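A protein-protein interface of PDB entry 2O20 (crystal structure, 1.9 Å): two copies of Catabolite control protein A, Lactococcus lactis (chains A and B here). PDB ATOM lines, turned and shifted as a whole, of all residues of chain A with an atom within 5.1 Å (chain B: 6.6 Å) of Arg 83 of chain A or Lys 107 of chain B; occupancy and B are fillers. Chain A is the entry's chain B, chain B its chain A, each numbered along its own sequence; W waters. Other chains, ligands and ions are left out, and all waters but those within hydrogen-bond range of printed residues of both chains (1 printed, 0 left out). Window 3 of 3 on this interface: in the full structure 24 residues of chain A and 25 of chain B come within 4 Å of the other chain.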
ATOM      1  N   ALA A  79      -0.496  35.230  26.635  1.00  0.00           N
ATOM      2  CA  ALA A  79       0.103  33.878  26.507  1.00  0.00           C
ATOM      3  C   ALA A  79      -0.953  32.753  26.388  1.00  0.00           C
ATOM      4  O   ALA A  79      -0.774  31.797  25.619  1.00  0.00           O
ATOM      5  CB  ALA A  79       1.074  33.610  27.651  1.00  0.00           C
ATOM      6  N   ALA A  80      -2.068  32.861  27.123  1.00  0.00           N
ATOM      7  CA  ALA A  80      -3.103  31.849  27.053  1.00  0.00           C
ATOM      8  C   ALA A  80      -3.810  31.835  25.709  1.00  0.00           C
ATOM      9  O   ALA A  80      -4.074  30.767  25.154  1.00  0.00           O
ATOM     10  CB  ALA A  80      -4.094  32.034  28.192  1.00  0.00           C
ATOM     11  N   ILE A  81      -4.094  33.004  25.172  1.00  0.00           N
ATOM     12  CA  ILE A  81      -4.614  33.134  23.816  1.00  0.00           C
ATOM     13  C   ILE A  81      -3.675  32.538  22.779  1.00  0.00           C
ATOM     14  O   ILE A  81      -4.102  31.805  21.863  1.00  0.00           O
ATOM     15  CB  ILE A  81      -4.915  34.623  23.438  1.00  0.00           C
ATOM     16  CG1 ILE A  81      -6.020  35.190  24.344  1.00  0.00           C
ATOM     17  CG2 ILE A  81      -5.339  34.729  21.970  1.00  0.00           C
ATOM     18  CD1 ILE A  81      -6.138  36.692  24.266  1.00  0.00           C
ATOM     19  N   THR A  82      -2.396  32.843  22.946  1.00  0.00           N
ATOM     20  CA  THR A  82      -1.351  32.438  22.016  1.00  0.00           C
ATOM     21  C   THR A  82      -1.260  30.903  21.960  1.00  0.00           C
ATOM     22  O   THR A  82      -1.029  30.346  20.874  1.00  0.00           O
ATOM     23  CB  THR A  82       0.019  33.147  22.341  1.00  0.00           C
ATOM     24  OG1 THR A  82      -0.104  34.582  22.214  1.00  0.00           O
ATOM     25  CG2 THR A  82       1.117  32.696  21.426  1.00  0.00           C
ATOM     26  N   ARG A  83      -1.467  30.202  23.075  1.00  0.00           N
ATOM     27  CA  ARG A  83      -1.465  28.724  23.038  1.00  0.00           C
ATOM     28  C   ARG A  83      -2.606  28.150  22.177  1.00  0.00           C
ATOM     29  O   ARG A  83      -2.420  27.124  21.508  1.00  0.00           O
ATOM     30  CB  ARG A  83      -1.427  28.094  24.440  1.00  0.00           C
ATOM     31  CG  ARG A  83      -0.076  28.393  25.175  1.00  0.00           C
ATOM     32  CD  ARG A  83       0.457  27.307  26.074  1.00  0.00           C
ATOM     33  NE  ARG A  83       0.585  26.026  25.395  1.00  0.00           N
ATOM     34  CZ  ARG A  83       0.824  24.876  26.012  1.00  0.00           C
ATOM     35  NH1 ARG A  83       1.004  24.827  27.332  1.00  0.00           N
ATOM     36  NH2 ARG A  83       0.892  23.761  25.305  1.00  0.00           N
ATOM     37  N   GLY A  84      -3.752  28.826  22.153  1.00  0.00           N
ATOM     38  CA  GLY A  84      -4.869  28.409  21.275  1.00  0.00           C
ATOM     39  C   GLY A  84      -4.542  28.582  19.794  1.00  0.00           C
ATOM     40  O   GLY A  84      -4.844  27.715  18.947  1.00  0.00           O
ATOM     41  N   VAL A  85      -3.915  29.702  19.471  1.00  0.00           N
ATOM     42  CA  VAL A  85      -3.391  29.964  18.118  1.00  0.00           C
ATOM     43  C   VAL A  85      -2.371  28.885  17.703  1.00  0.00           C
ATOM     44  O   VAL A  85      -2.500  28.265  16.625  1.00  0.00           O
ATOM     45  CB  VAL A  85      -2.724  31.364  18.030  1.00  0.00           C
ATOM     46  CG1 VAL A  85      -2.087  31.619  16.635  1.00  0.00           C
ATOM     47  CG2 VAL A  85      -3.698  32.469  18.366  1.00  0.00           C
ATOM     48  N   ASP A  86      -1.371  28.671  18.562  1.00  0.00           N
ATOM     49  CA  ASP A  86      -0.297  27.699  18.331  1.00  0.00           C
ATOM     50  C   ASP A  86      -0.816  26.282  18.046  1.00  0.00           C
ATOM     51  O   ASP A  86      -0.349  25.614  17.124  1.00  0.00           O
ATOM     52  CB  ASP A  86       0.626  27.702  19.551  1.00  0.00           C
ATOM     53  CG  ASP A  86       1.868  26.841  19.379  1.00  0.00           C
ATOM     54  OD1 ASP A  86       2.189  26.064  20.312  1.00  0.00           O
ATOM     55  OD2 ASP A  86       2.531  26.966  18.339  1.00  0.00           O
ATOM     56  N   ASP A  87      -1.775  25.819  18.855  1.00  0.00           N
ATOM     57  CA  ASP A  87      -2.321  24.491  18.696  1.00  0.00           C
ATOM     58  C   ASP A  87      -2.990  24.263  17.333  1.00  0.00           C
ATOM     59  O   ASP A  87      -2.800  23.187  16.710  1.00  0.00           O
ATOM     60  CB  ASP A  87      -3.256  24.165  19.860  1.00  0.00           C
ATOM     61  CG  ASP A  87      -2.489  23.760  21.120  1.00  0.00           C
ATOM     62  OD1 ASP A  87      -1.234  23.828  21.079  1.00  0.00           O
ATOM     63  OD2 ASP A  87      -3.139  23.420  22.153  1.00  0.00           O
ATOM     64  N   TYR A 295      -8.109  30.470  25.685  1.00  0.00           N
ATOM     65  CA  TYR A 295      -7.656  29.487  24.707  1.00  0.00           C
ATOM     66  C   TYR A 295      -8.550  29.467  23.456  1.00  0.00           C
ATOM     67  O   TYR A 295      -8.063  29.455  22.340  1.00  0.00           O
ATOM     68  CB  TYR A 295      -7.626  28.099  25.341  1.00  0.00           C
ATOM     69  CG  TYR A 295      -7.148  27.004  24.403  1.00  0.00           C
ATOM     70  CD1 TYR A 295      -5.805  26.684  24.329  1.00  0.00           C
ATOM     71  CD2 TYR A 295      -8.037  26.291  23.609  1.00  0.00           C
ATOM     72  CE1 TYR A 295      -5.355  25.677  23.485  1.00  0.00           C
ATOM     73  CE2 TYR A 295      -7.595  25.282  22.751  1.00  0.00           C
ATOM     74  CZ  TYR A 295      -6.242  24.990  22.696  1.00  0.00           C
ATOM     75  OH  TYR A 295      -5.783  23.990  21.862  1.00  0.00           O
ATOM     76  N   PRO B  71       8.211  24.487  29.334  1.00  0.00           N
ATOM     77  CA  PRO B  71       6.948  23.761  29.574  1.00  0.00           C
ATOM     78  C   PRO B  71       5.673  24.484  29.070  1.00  0.00           C
ATOM     79  O   PRO B  71       4.847  23.886  28.390  1.00  0.00           O
ATOM     80  CB  PRO B  71       6.955  23.569  31.094  1.00  0.00           C
ATOM     81  CG  PRO B  71       8.420  23.547  31.429  1.00  0.00           C
ATOM     82  CD  PRO B  71       8.973  24.652  30.574  1.00  0.00           C
ATOM     83  N   THR B  72       5.553  25.780  29.376  1.00  0.00           N
ATOM     84  CA  THR B  72       4.398  26.563  28.972  1.00  0.00           C
ATOM     85  C   THR B  72       4.681  28.067  29.092  1.00  0.00           C
ATOM     86  O   THR B  72       5.222  28.532  30.110  1.00  0.00           O
ATOM     87  CB  THR B  72       3.098  26.188  29.731  1.00  0.00           C
ATOM     88  OG1 THR B  72       2.024  27.016  29.276  1.00  0.00           O
ATOM     89  CG2 THR B  72       3.231  26.262  31.267  1.00  0.00           C
ATOM     90  N   ILE B  73       4.330  28.802  28.033  1.00  0.00           N
ATOM     91  CA  ILE B  73       4.404  30.258  28.071  1.00  0.00           C
ATOM     92  C   ILE B  73       3.440  30.892  29.081  1.00  0.00           C
ATOM     93  O   ILE B  73       3.575  32.068  29.395  1.00  0.00           O
ATOM     94  CB  ILE B  73       4.224  30.926  26.681  1.00  0.00           C
ATOM     95  CG1 ILE B  73       2.961  30.442  25.980  1.00  0.00           C
ATOM     96  CG2 ILE B  73       5.477  30.716  25.841  1.00  0.00           C
ATOM     97  CD1 ILE B  73       2.585  31.310  24.812  1.00  0.00           C
ATOM     98  N   THR B  74       2.477  30.132  29.590  1.00  0.00           N
ATOM     99  CA  THR B  74       1.590  30.641  30.643  1.00  0.00           C
ATOM    100  C   THR B  74       2.201  30.644  32.064  1.00  0.00           C
ATOM    101  O   THR B  74       1.580  31.197  32.981  1.00  0.00           O
ATOM    102  CB  THR B  74       0.186  29.960  30.653  1.00  0.00           C
ATOM    103  OG1 THR B  74       0.307  28.543  30.896  1.00  0.00           O
ATOM    104  CG2 THR B  74      -0.549  30.213  29.358  1.00  0.00           C
ATOM    105  N   ASN B 100       6.118  24.764  23.268  1.00  0.00           N
ATOM    106  CA  ASN B 100       5.641  24.412  24.616  1.00  0.00           C
ATOM    107  C   ASN B 100       5.678  22.888  24.759  1.00  0.00           C
ATOM    108  O   ASN B 100       5.035  22.173  23.995  1.00  0.00           O
ATOM    109  CB  ASN B 100       4.216  24.921  24.833  1.00  0.00           C
ATOM    110  CG  ASN B 100       4.099  26.424  24.737  1.00  0.00           C
ATOM    111  OD1 ASN B 100       4.341  27.152  25.707  1.00  0.00           O
ATOM    112  ND2 ASN B 100       3.708  26.906  23.574  1.00  0.00           N
ATOM    113  N   SER B 101       6.438  22.387  25.715  1.00  0.00           N
ATOM    114  CA  SER B 101       6.558  20.927  25.945  1.00  0.00           C
ATOM    115  C   SER B 101       5.518  20.319  26.892  1.00  0.00           C
ATOM    116  O   SER B 101       5.283  19.103  26.862  1.00  0.00           O
ATOM    117  CB  SER B 101       7.921  20.617  26.514  1.00  0.00           C
ATOM    118  OG  SER B 101       8.030  21.050  27.856  1.00  0.00           O
ATOM    119  N   ASP B 102       4.934  21.158  27.751  1.00  0.00           N
ATOM    120  CA  ASP B 102       4.124  20.726  28.894  1.00  0.00           C
ATOM    121  C   ASP B 102       4.795  19.678  29.795  1.00  0.00           C
ATOM    122  O   ASP B 102       4.105  18.870  30.402  1.00  0.00           O
ATOM    123  CB  ASP B 102       2.755  20.210  28.410  1.00  0.00           C
ATOM    124  CG  ASP B 102       1.930  21.290  27.756  1.00  0.00           C
ATOM    125  OD1 ASP B 102       1.687  22.328  28.408  1.00  0.00           O
ATOM    126  OD2 ASP B 102       1.537  21.110  26.594  1.00  0.00           O
ATOM    127  N   ASN B 103       6.126  19.676  29.836  1.00  0.00           N
ATOM    128  CA  ASN B 103       6.951  18.695  30.548  1.00  0.00           C
ATOM    129  C   ASN B 103       6.756  17.234  30.110  1.00  0.00           C
ATOM    130  O   ASN B 103       6.971  16.313  30.909  1.00  0.00           O
ATOM    131  CB  ASN B 103       6.770  18.845  32.083  1.00  0.00           C
ATOM    132  CG  ASN B 103       7.484  20.081  32.645  1.00  0.00           C
ATOM    133  OD1 ASN B 103       6.898  20.862  33.383  1.00  0.00           O
ATOM    134  ND2 ASN B 103       8.748  20.269  32.267  1.00  0.00           N
ATOM    135  N   ASP B 104       6.343  17.030  28.857  1.00  0.00           N
ATOM    136  CA  ASP B 104       6.022  15.686  28.304  1.00  0.00           C
ATOM    137  C   ASP B 104       7.243  15.280  27.481  1.00  0.00           C
ATOM    138  O   ASP B 104       7.593  15.958  26.526  1.00  0.00           O
ATOM    139  CB  ASP B 104       4.752  15.833  27.455  1.00  0.00           C
ATOM    140  CG  ASP B 104       4.367  14.583  26.662  1.00  0.00           C
ATOM    141  OD1 ASP B 104       5.157  13.634  26.472  1.00  0.00           O
ATOM    142  OD2 ASP B 104       3.208  14.587  26.195  1.00  0.00           O
ATOM    143  N   VAL B 105       7.929  14.215  27.886  1.00  0.00           N
ATOM    144  CA  VAL B 105       9.185  13.808  27.243  1.00  0.00           C
ATOM    145  C   VAL B 105       8.982  13.386  25.800  1.00  0.00           C
ATOM    146  O   VAL B 105       9.835  13.650  24.952  1.00  0.00           O
ATOM    147  CB  VAL B 105       9.918  12.673  28.035  1.00  0.00           C
ATOM    148  CG1 VAL B 105      11.142  12.192  27.283  1.00  0.00           C
ATOM    149  CG2 VAL B 105      10.344  13.178  29.421  1.00  0.00           C
ATOM    150  N   GLU B 106       7.849  12.744  25.516  1.00  0.00           N
ATOM    151  CA  GLU B 106       7.500  12.401  24.142  1.00  0.00           C
ATOM    152  C   GLU B 106       7.340  13.652  23.284  1.00  0.00           C
ATOM    153  O   GLU B 106       7.804  13.685  22.157  1.00  0.00           O
ATOM    154  CB  GLU B 106       6.228  11.559  24.086  1.00  0.00           C
ATOM    155  CG  GLU B 106       6.372  10.226  24.809  1.00  0.00           C
ATOM    156  CD  GLU B 106       5.305   9.199  24.422  1.00  0.00           C
ATOM    157  OE1 GLU B 106       5.679   8.209  23.753  1.00  0.00           O
ATOM    158  OE2 GLU B 106       4.104   9.370  24.780  1.00  0.00           O
ATOM    159  N   LYS B 107       6.697  14.677  23.826  1.00  0.00           N
ATOM    160  CA  LYS B 107       6.571  15.948  23.114  1.00  0.00           C
ATOM    161  C   LYS B 107       7.933  16.622  22.893  1.00  0.00           C
ATOM    162  O   LYS B 107       8.210  17.115  21.800  1.00  0.00           O
ATOM    163  CB  LYS B 107       5.623  16.906  23.852  1.00  0.00           C
ATOM    164  CG  LYS B 107       5.108  17.976  22.947  1.00  0.00           C
ATOM    165  CD  LYS B 107       4.410  19.120  23.662  1.00  0.00           C
ATOM    166  CE  LYS B 107       2.938  18.881  23.996  1.00  0.00           C
ATOM    167  NZ  LYS B 107       2.292  20.228  24.066  1.00  0.00           N
ATOM    168  N   GLU B 108       8.770  16.652  23.929  1.00  0.00           N
ATOM    169  CA  GLU B 108      10.124  17.200  23.815  1.00  0.00           C
ATOM    170  C   GLU B 108      10.922  16.514  22.722  1.00  0.00           C
ATOM    171  O   GLU B 108      11.585  17.186  21.927  1.00  0.00           O
ATOM    172  CB  GLU B 108      10.891  17.097  25.139  1.00  0.00           C
ATOM    173  CG  GLU B 108      10.290  17.921  26.246  1.00  0.00           C
ATOM    174  CD  GLU B 108      10.985  17.767  27.574  1.00  0.00           C
ATOM    175  OE1 GLU B 108      11.452  16.656  27.907  1.00  0.00           O
ATOM    176  OE2 GLU B 108      11.046  18.788  28.303  1.00  0.00           O
ATOM    177  N   GLU B 109      10.820  15.186  22.644  1.00  0.00           N
ATOM    178  CA  GLU B 109      11.509  14.447  21.596  1.00  0.00           C
ATOM    179  C   GLU B 109      11.085  14.884  20.194  1.00  0.00           C
ATOM    180  O   GLU B 109      11.937  15.098  19.331  1.00  0.00           O
ATOM    181  CB  GLU B 109      11.290  12.945  21.746  1.00  0.00           C
ATOM    182  CG  GLU B 109      12.098  12.320  22.864  1.00  0.00           C
ATOM    183  CD  GLU B 109      11.897  10.811  22.946  1.00  0.00           C
ATOM    184  OE1 GLU B 109      12.922  10.100  23.063  1.00  0.00           O
ATOM    185  OE2 GLU B 109      10.733  10.332  22.856  1.00  0.00           O
ATOM    186  N   LYS B 110       9.778  15.039  19.992  1.00  0.00           N
ATOM    187  CA  LYS B 110       9.211  15.444  18.693  1.00  0.00           C
ATOM    188  C   LYS B 110       9.602  16.880  18.314  1.00  0.00           C
ATOM    189  O   LYS B 110       9.898  17.182  17.161  1.00  0.00           O
ATOM    190  CB  LYS B 110       7.696  15.350  18.760  1.00  0.00           C
ATOM    191  CG  LYS B 110       6.988  15.545  17.433  1.00  0.00           C
ATOM    192  CD  LYS B 110       5.520  15.096  17.531  1.00  0.00           C
ATOM    193  CE  LYS B 110       4.813  15.124  16.178  1.00  0.00           C
ATOM    194  NZ  LYS B 110       5.088  16.430  15.482  1.00  0.00           N
ATOM    195  N   VAL B 111       9.585  17.758  19.305  1.00  0.00           N
ATOM    196  CA  VAL B 111      10.032  19.143  19.126  1.00  0.00           C
ATOM    197  C   VAL B 111      11.489  19.206  18.629  1.00  0.00           C
ATOM    198  O   VAL B 111      11.818  19.962  17.697  1.00  0.00           O
ATOM    199  CB  VAL B 111       9.880  19.931  20.438  1.00  0.00           C
ATOM    200  CG1 VAL B 111      10.710  21.230  20.404  1.00  0.00           C
ATOM    201  CG2 VAL B 111       8.427  20.195  20.708  1.00  0.00           C
ATOM    202  N   LEU B 112      12.376  18.442  19.250  1.00  0.00           N
ATOM    203  CA  LEU B 112      13.763  18.428  18.800  1.00  0.00           C
ATOM    204  C   LEU B 112      13.912  17.936  17.365  1.00  0.00           C
ATOM    205  O   LEU B 112      14.737  18.472  16.612  1.00  0.00           O
ATOM    206  CB  LEU B 112      14.657  17.604  19.731  1.00  0.00           C
ATOM    207  CG  LEU B 112      14.907  18.223  21.100  1.00  0.00           C
ATOM    208  CD1 LEU B 112      15.788  17.267  21.918  1.00  0.00           C
ATOM    209  CD2 LEU B 112      15.550  19.594  20.960  1.00  0.00           C
ATOM    210  N   ILE B 134      16.421  13.130  26.324  1.00  0.00           N
ATOM    211  CA  ILE B 134      16.592  14.470  25.768  1.00  0.00           C
ATOM    212  C   ILE B 134      18.090  14.845  25.677  1.00  0.00           C
ATOM    213  O   ILE B 134      18.528  15.413  24.672  1.00  0.00           O
ATOM    214  CB  ILE B 134      15.728  15.501  26.531  1.00  0.00           C
ATOM    215  CG1 ILE B 134      14.254  15.041  26.568  1.00  0.00           C
ATOM    216  CG2 ILE B 134      15.827  16.863  25.874  1.00  0.00           C
ATOM    217  CD1 ILE B 134      13.644  14.658  25.197  1.00  0.00           C
HETATM  218  O   HOH W   1       4.119  24.776  21.058  1.00  0.00           O
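The side-chain hydroxyl of Thr 72 of chain B is in hydrogen-bond range of the guanidinium group of Arg 83 of chain A. NH1 of Arg 83 of chain A is in salt-bridge range of OD1 of Asp 102 of chain B (2.8 Å).
The backbone NH (N) of Asp 102 of chain B is in hydrogen-bond range of the backbone carbonyl oxygen (O) of Pro 71 of chain B, at 2.8 Å. OG1 of Thr 72 of chain B sits at hydrogen-bond distance from OG1 of Thr 74 of chain B (2.8 Å). The side-chain amide oxygen (OD1) of Asn 100 of chain B lies within hydrogen-bond range of the backbone NH (N) of Ile 73 of chain B (2.9 Å). The backbone carbonyl oxygen of Asn 100 of chain B lies close to the side-chain amino group of Lys 107 of chain B (3.4 Å). The side-chain carboxylate (OD2) of Asp 102 of chain B lies within salt-bridge range of the side-chain amino group (NZ) of Lys 107 of chain B (2.8 Å). The backbone NH of Lys 107 of chain B sits at hydrogen-bond distance from the side-chain carboxylate of Asp 104 of chain B (3.2 Å).
CB of Ala 79 of chain A touches O of Ile 73 of chain B (3.4 Å). Ala 79 of chain A touches Thr 74 of chain B (C to CG2, 3.9 Å). Ala 80 of chain A touches Thr 74 of chain B (N to CG2, 3.8 Å). Thr 82 of chain A touches Ile 73 of chain B. CG of Arg 83 of chain A touches CG1 of Ile 73 of chain B, at 3.8 Å. Asn 100 of chain B touches Arg 83 of chain A (CB to NH2, 3.6 Å). NZ of Lys 107 of chain B touches NH2 of Arg 83 of chain A (3.997 Å). Asp 86 of chain A touches Asn 100 of chain B.
Of the printed residues of chain B, Thr 82 of chain A touches Ile 73. Printed residues of chain B within 4 Å of Arg 83 of chain A: Thr 72, Ile 73, Asn 100, Asp 102 and Lys 107. Val 85 of chain A touches none of the printed residues of chain B. Printed residues of chain A within 4 Å of Ile 73 of chain B: Ala 79 (3.4 Å), Thr 82 (3.9 Å) and Arg 83 (3.8 Å). Of the printed residues of chain A, Asn 100 of chain B touches Arg 83 (3.6 Å) and Asp 86 (3.7 Å). Printed residues of chain A within 4 Å of Asp 102 of chain B: Arg 83 (2.8 Å). Of the printed residues of chain A, Lys 107 of chain B touches Arg 83. Glu 109 of chain B touches none of the printed residues of chain A. The nearest printed residue of chain A that does not touch Lys 107 of chain B is Asp 87 of chain A (5.9 Å).
Of the 18 printed residues of chain B, 6 touch a printed residue of chain A. Hydrophobic or aromatic side chains of chain B that line the printed part of chain A: Ile 73. Of the 10 printed residues of chain A, 5 touch a printed residue of chain B. Hydrophobic or aromatic side chains of chain A that line the printed part of chain B: Ala 79.
No position is printed for both chains.
Water W1 bridges the side-chain carboxylate (OD1) of Asp 86 of chain A (2.4 Å) and the backbone NH (N) of Asn 100 of chain B (3.0 Å).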
